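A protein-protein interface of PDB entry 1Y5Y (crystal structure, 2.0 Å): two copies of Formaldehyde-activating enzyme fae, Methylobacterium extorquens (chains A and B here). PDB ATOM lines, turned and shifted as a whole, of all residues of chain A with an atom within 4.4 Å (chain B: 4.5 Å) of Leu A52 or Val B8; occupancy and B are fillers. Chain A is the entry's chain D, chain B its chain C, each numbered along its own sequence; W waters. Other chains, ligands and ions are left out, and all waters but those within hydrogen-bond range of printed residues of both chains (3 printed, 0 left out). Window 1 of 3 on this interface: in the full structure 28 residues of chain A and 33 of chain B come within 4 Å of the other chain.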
ATOM      1  N   PHE A  37      31.256 -24.342  -0.884  1.00  0.00           N
ATOM      2  CA  PHE A  37      29.902 -24.810  -0.566  1.00  0.00           C
ATOM      3  C   PHE A  37      29.938 -25.838   0.603  1.00  0.00           C
ATOM      4  O   PHE A  37      29.197 -25.719   1.591  1.00  0.00           O
ATOM      5  CB  PHE A  37      29.295 -25.516  -1.798  1.00  0.00           C
ATOM      6  CG  PHE A  37      27.929 -26.076  -1.560  1.00  0.00           C
ATOM      7  CD1 PHE A  37      26.798 -25.329  -1.868  1.00  0.00           C
ATOM      8  CD2 PHE A  37      27.770 -27.364  -1.033  1.00  0.00           C
ATOM      9  CE1 PHE A  37      25.496 -25.836  -1.661  1.00  0.00           C
ATOM     10  CE2 PHE A  37      26.494 -27.876  -0.825  1.00  0.00           C
ATOM     11  CZ  PHE A  37      25.349 -27.092  -1.148  1.00  0.00           C
ATOM     12  N   LEU A  41      28.676 -25.173   4.450  1.00  0.00           N
ATOM     13  CA  LEU A  41      27.529 -25.837   5.071  1.00  0.00           C
ATOM     14  C   LEU A  41      27.960 -26.390   6.460  1.00  0.00           C
ATOM     15  O   LEU A  41      27.207 -26.413   7.414  1.00  0.00           O
ATOM     16  CB  LEU A  41      27.101 -27.018   4.161  1.00  0.00           C
ATOM     17  CG  LEU A  41      25.863 -27.781   4.677  1.00  0.00           C
ATOM     18  CD1 LEU A  41      24.624 -26.855   4.555  1.00  0.00           C
ATOM     19  CD2 LEU A  41      25.658 -29.055   3.819  1.00  0.00           C
ATOM     20  N   LEU A  51      22.411 -22.328   5.185  1.00  0.00           N
ATOM     21  CA  LEU A  51      21.478 -23.413   4.937  1.00  0.00           C
ATOM     22  C   LEU A  51      21.425 -23.794   3.487  1.00  0.00           C
ATOM     23  O   LEU A  51      21.856 -23.034   2.605  1.00  0.00           O
ATOM     24  CB  LEU A  51      20.067 -23.113   5.458  1.00  0.00           C
ATOM     25  CG  LEU A  51      19.274 -21.813   5.332  1.00  0.00           C
ATOM     26  CD1 LEU A  51      19.899 -20.762   6.229  1.00  0.00           C
ATOM     27  CD2 LEU A  51      19.168 -21.380   3.884  1.00  0.00           C
ATOM     28  N   LEU A  52      20.920 -24.993   3.260  1.00  0.00           N
ATOM     29  CA  LEU A  52      20.774 -25.554   1.931  1.00  0.00           C
ATOM     30  C   LEU A  52      19.382 -25.000   1.591  1.00  0.00           C
ATOM     31  O   LEU A  52      18.361 -25.393   2.177  1.00  0.00           O
ATOM     32  CB  LEU A  52      20.716 -27.069   2.048  1.00  0.00           C
ATOM     33  CG  LEU A  52      21.477 -28.008   1.151  1.00  0.00           C
ATOM     34  CD1 LEU A  52      22.922 -27.485   0.926  1.00  0.00           C
ATOM     35  CD2 LEU A  52      21.480 -29.404   1.838  1.00  0.00           C
ATOM     36  N   ALA A  53      19.328 -24.086   0.647  1.00  0.00           N
ATOM     37  CA  ALA A  53      18.040 -23.428   0.326  1.00  0.00           C
ATOM     38  C   ALA A  53      16.969 -24.323  -0.296  1.00  0.00           C
ATOM     39  O   ALA A  53      17.262 -25.080  -1.223  1.00  0.00           O
ATOM     40  CB  ALA A  53      18.289 -22.253  -0.595  1.00  0.00           C
ATOM     41  N   VAL A  54      15.729 -24.212   0.185  1.00  0.00           N
ATOM     42  CA  VAL A  54      14.670 -25.037  -0.390  1.00  0.00           C
ATOM     43  C   VAL A  54      13.506 -24.196  -0.840  1.00  0.00           C
ATOM     44  O   VAL A  54      13.248 -23.137  -0.255  1.00  0.00           O
ATOM     45  CB  VAL A  54      14.126 -26.114   0.627  1.00  0.00           C
ATOM     46  CG1 VAL A  54      15.295 -26.867   1.270  1.00  0.00           C
ATOM     47  CG2 VAL A  54      13.274 -25.446   1.747  1.00  0.00           C
ATOM     48  N   ASN A  64      22.303 -26.874  -6.270  1.00  0.00           N
ATOM     49  CA  ASN A  64      22.561 -26.813  -4.837  1.00  0.00           C
ATOM     50  C   ASN A  64      22.926 -25.372  -4.480  1.00  0.00           C
ATOM     51  O   ASN A  64      23.865 -24.815  -5.038  1.00  0.00           O
ATOM     52  CB  ASN A  64      23.744 -27.723  -4.488  1.00  0.00           C
ATOM     53  CG  ASN A  64      23.408 -29.207  -4.650  1.00  0.00           C
ATOM     54  OD1 ASN A  64      22.337 -29.648  -4.245  1.00  0.00           O
ATOM     55  ND2 ASN A  64      24.341 -29.972  -5.207  1.00  0.00           N
ATOM     56  N   THR A  65      22.217 -24.821  -3.514  1.00  0.00           N
ATOM     57  CA  THR A  65      22.415 -23.449  -3.094  1.00  0.00           C
ATOM     58  C   THR A  65      22.627 -23.328  -1.583  1.00  0.00           C
ATOM     59  O   THR A  65      21.799 -23.777  -0.780  1.00  0.00           O
ATOM     60  CB  THR A  65      21.161 -22.644  -3.483  1.00  0.00           C
ATOM     61  OG1 THR A  65      21.061 -22.609  -4.918  1.00  0.00           O
ATOM     62  CG2 THR A  65      21.222 -21.199  -2.942  1.00  0.00           C
ATOM     63  N   GLN A  87      14.775 -16.949   2.371  1.00  0.00           N
ATOM     64  CA  GLN A  87      15.093 -18.256   1.815  1.00  0.00           C
ATOM     65  C   GLN A  87      14.169 -18.568   0.627  1.00  0.00           C
ATOM     66  O   GLN A  87      14.623 -19.023  -0.432  1.00  0.00           O
ATOM     67  CB  GLN A  87      14.935 -19.381   2.871  1.00  0.00           C
ATOM     68  CG  GLN A  87      15.177 -20.772   2.211  1.00  0.00           C
ATOM     69  CD  GLN A  87      15.207 -21.962   3.178  1.00  0.00           C
ATOM     70  OE1 GLN A  87      15.723 -23.014   2.806  1.00  0.00           O
ATOM     71  NE2 GLN A  87      14.653 -21.811   4.393  1.00  0.00           N
ATOM     72  N   GLN B   7      27.896 -35.507  -3.402  1.00  0.00           N
ATOM     73  CA  GLN B   7      26.441 -35.386  -3.565  1.00  0.00           C
ATOM     74  C   GLN B   7      25.875 -34.733  -2.299  1.00  0.00           C
ATOM     75  O   GLN B   7      26.399 -34.914  -1.198  1.00  0.00           O
ATOM     76  CB  GLN B   7      25.769 -36.755  -3.726  1.00  0.00           C
ATOM     77  CG  GLN B   7      26.291 -37.548  -4.916  1.00  0.00           C
ATOM     78  CD  GLN B   7      26.020 -36.892  -6.250  1.00  0.00           C
ATOM     79  OE1 GLN B   7      25.076 -36.102  -6.425  1.00  0.00           O
ATOM     80  NE2 GLN B   7      26.867 -37.213  -7.215  1.00  0.00           N
ATOM     81  N   VAL B   8      24.761 -34.039  -2.472  1.00  0.00           N
ATOM     82  CA  VAL B   8      24.106 -33.303  -1.409  1.00  0.00           C
ATOM     83  C   VAL B   8      22.684 -33.783  -1.234  1.00  0.00           C
ATOM     84  O   VAL B   8      21.961 -33.928  -2.220  1.00  0.00           O
ATOM     85  CB  VAL B   8      24.091 -31.794  -1.788  1.00  0.00           C
ATOM     86  CG1 VAL B   8      23.505 -30.980  -0.656  1.00  0.00           C
ATOM     87  CG2 VAL B   8      25.525 -31.350  -2.092  1.00  0.00           C
ATOM     88  N   GLY B   9      22.288 -34.023   0.015  1.00  0.00           N
ATOM     89  CA  GLY B   9      20.935 -34.471   0.308  1.00  0.00           C
ATOM     90  C   GLY B   9      20.372 -33.713   1.495  1.00  0.00           C
ATOM     91  O   GLY B   9      21.123 -33.098   2.264  1.00  0.00           O
ATOM     92  N   GLU B  10      19.056 -33.755   1.640  1.00  0.00           N
ATOM     93  CA  GLU B  10      18.386 -33.093   2.743  1.00  0.00           C
ATOM     94  C   GLU B  10      17.010 -33.693   2.937  1.00  0.00           C
ATOM     95  O   GLU B  10      16.452 -34.328   2.043  1.00  0.00           O
ATOM     96  CB  GLU B  10      18.272 -31.559   2.499  1.00  0.00           C
ATOM     97  CG  GLU B  10      17.240 -31.143   1.553  1.00  0.00           C
ATOM     98  CD  GLU B  10      15.829 -31.013   2.183  1.00  0.00           C
ATOM     99  OE1 GLU B  10      14.927 -31.548   1.529  1.00  0.00           O
ATOM    100  OE2 GLU B  10      15.603 -30.400   3.280  1.00  0.00           O
ATOM    101  N   ASP B  23      20.823 -31.823   6.707  1.00  0.00           N
ATOM    102  CA  ASP B  23      21.501 -31.353   5.489  1.00  0.00           C
ATOM    103  C   ASP B  23      22.651 -32.341   5.429  1.00  0.00           C
ATOM    104  O   ASP B  23      23.292 -32.627   6.451  1.00  0.00           O
ATOM    105  CB  ASP B  23      22.078 -29.936   5.616  1.00  0.00           C
ATOM    106  CG  ASP B  23      21.013 -28.879   5.656  1.00  0.00           C
ATOM    107  OD1 ASP B  23      19.902 -29.110   5.118  1.00  0.00           O
ATOM    108  OD2 ASP B  23      21.297 -27.801   6.206  1.00  0.00           O
ATOM    109  N   LEU B  24      22.958 -32.832   4.243  1.00  0.00           N
ATOM    110  CA  LEU B  24      23.957 -33.879   4.170  1.00  0.00           C
ATOM    111  C   LEU B  24      24.789 -33.884   2.926  1.00  0.00           C
ATOM    112  O   LEU B  24      24.301 -33.617   1.824  1.00  0.00           O
ATOM    113  CB  LEU B  24      23.233 -35.224   4.312  1.00  0.00           C
ATOM    114  CG  LEU B  24      24.026 -36.526   4.352  1.00  0.00           C
ATOM    115  CD1 LEU B  24      23.242 -37.524   5.191  1.00  0.00           C
ATOM    116  CD2 LEU B  24      24.296 -37.065   2.936  1.00  0.00           C
ATOM    117  N   ILE B  25      26.059 -34.227   3.101  1.00  0.00           N
ATOM    118  CA  ILE B  25      26.991 -34.313   1.999  1.00  0.00           C
ATOM    119  C   ILE B  25      27.669 -35.674   2.055  1.00  0.00           C
ATOM    120  O   ILE B  25      28.000 -36.149   3.123  1.00  0.00           O
ATOM    121  CB  ILE B  25      28.077 -33.199   2.098  1.00  0.00           C
ATOM    122  CG1 ILE B  25      27.403 -31.823   1.864  1.00  0.00           C
ATOM    123  CG2 ILE B  25      29.156 -33.376   0.991  1.00  0.00           C
ATOM    124  CD1 ILE B  25      28.386 -30.623   2.014  1.00  0.00           C
ATOM    125  N   ALA B 144      20.736 -38.021  -1.681  1.00  0.00           N
ATOM    126  CA  ALA B 144      22.057 -37.605  -2.131  1.00  0.00           C
ATOM    127  C   ALA B 144      22.696 -38.618  -3.085  1.00  0.00           C
ATOM    128  O   ALA B 144      23.183 -38.267  -4.152  1.00  0.00           O
ATOM    129  CB  ALA B 144      22.990 -37.408  -0.908  1.00  0.00           C
ATOM    130  N   GLU B 148      18.941 -36.795  -6.081  1.00  0.00           N
ATOM    131  CA  GLU B 148      17.584 -36.238  -6.054  1.00  0.00           C
ATOM    132  C   GLU B 148      17.503 -35.097  -5.056  1.00  0.00           C
ATOM    133  O   GLU B 148      18.199 -35.107  -4.037  1.00  0.00           O
ATOM    134  CB  GLU B 148      16.550 -37.257  -5.602  1.00  0.00           C
ATOM    135  CG  GLU B 148      16.745 -38.696  -6.007  1.00  0.00           C
ATOM    136  CD  GLU B 148      16.027 -39.603  -5.008  1.00  0.00           C
ATOM    137  OE1 GLU B 148      16.392 -40.779  -4.890  1.00  0.00           O
ATOM    138  OE2 GLU B 148      15.094 -39.104  -4.328  1.00  0.00           O
HETATM  139  O   HOH W   1      17.676 -27.544   3.864  1.00  0.00           O
HETATM  140  O   HOH W   2      19.517 -25.964   5.871  1.00  0.00           O
HETATM  141  O   HOH W   3      24.097 -33.202  -5.285  1.00  0.00           O
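Phe A37 touches Val B8 (CE2 to CG2, 3.8 Å). CD1 of Leu A41 touches OD2 of Asp B23, at 3.8 Å. CD1 of Ile B25 touches CD2 of Leu A41 (3.6 Å). Leu A52 touches Val B8. Gly B9 touches Leu A52 (O to CD2, 3.7 Å). Leu A52 touches Glu B10. CD2 of Leu A52 touches OD1 of Asp B23, 3.7 Å away. Asn A64 touches Val B8.
Of chain B, only Val B8 (3.6 Å), Gly B9 (3.7 Å), Glu B10 (3.9 Å) and Asp B23 (3.7 Å) come within 4 Å of Leu A52. Of chain A, only Phe A37, Leu A52 and Asn A64 come within 4 Å of Val B8. Printed residues of chain A within 4 Å of Ile B25: Leu A41. Of the printed residues of chain A, Gly B9 touches Leu A52. Of the printed residues of chain B, Asn A64 touches Val B8 (3.6 Å). Val A54 touches none of the printed residues of chain B. Ala A53 touches none of the printed residues of chain B. The nearest residue of chain B that does not touch Leu A52 is Leu B24 (4.4 Å). The nearest printed residue of chain A that does not touch Val B8 is Leu A41 (5.3 Å).
The backbone NH (N) of Leu B24 is in hydrogen-bond range of the backbone carbonyl oxygen (O) of Gly B9 (2.7 Å).
Of the 9 printed residues of chain B, 5 touch a printed residue of chain A. Printed residues of chain B that touch a printed residue of chain A: Val B8, Gly B9, Glu B10, Asp B23 and Ile B25. Hydrophobic or aromatic side chains of chain B within 4 Å of the printed part of chain A: Val B8 and Ile B25. Of the 9 printed residues of chain A, 4 touch a printed residue of chain B. Printed residues of chain A that touch a printed residue of chain B: Phe A37, Leu A41, Leu A52 and Asn A64. Hydrophobic or aromatic side chains of chain A within 4 Å of the printed part of chain B: Phe A37, Leu A41 and Leu A52. Among the printed residues, no Asp or Glu carboxylate lies within 4 Å of a Lys or Arg side-chain nitrogen of the other chain.
No position is printed for both chains. Of the 8 pairs that touch across the chains among the printed residues, none has its exchanged pair printed and touching as well.
Water W2 bridges the side-chain carboxylate of Asp B23 and the backbone NH of Leu A52. Water W1 bridges the backbone carbonyl oxygen (O) of Leu A52 (2.8 Å) and the side-chain carboxylate (OD1) of Asp B23 (3.0 Å). Water W3 lies within hydrogen-bond range of the backbone NH of Val B8, the side-chain amide nitrogen of Asn A64 and the side-chain amide oxygen of Gln B7.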
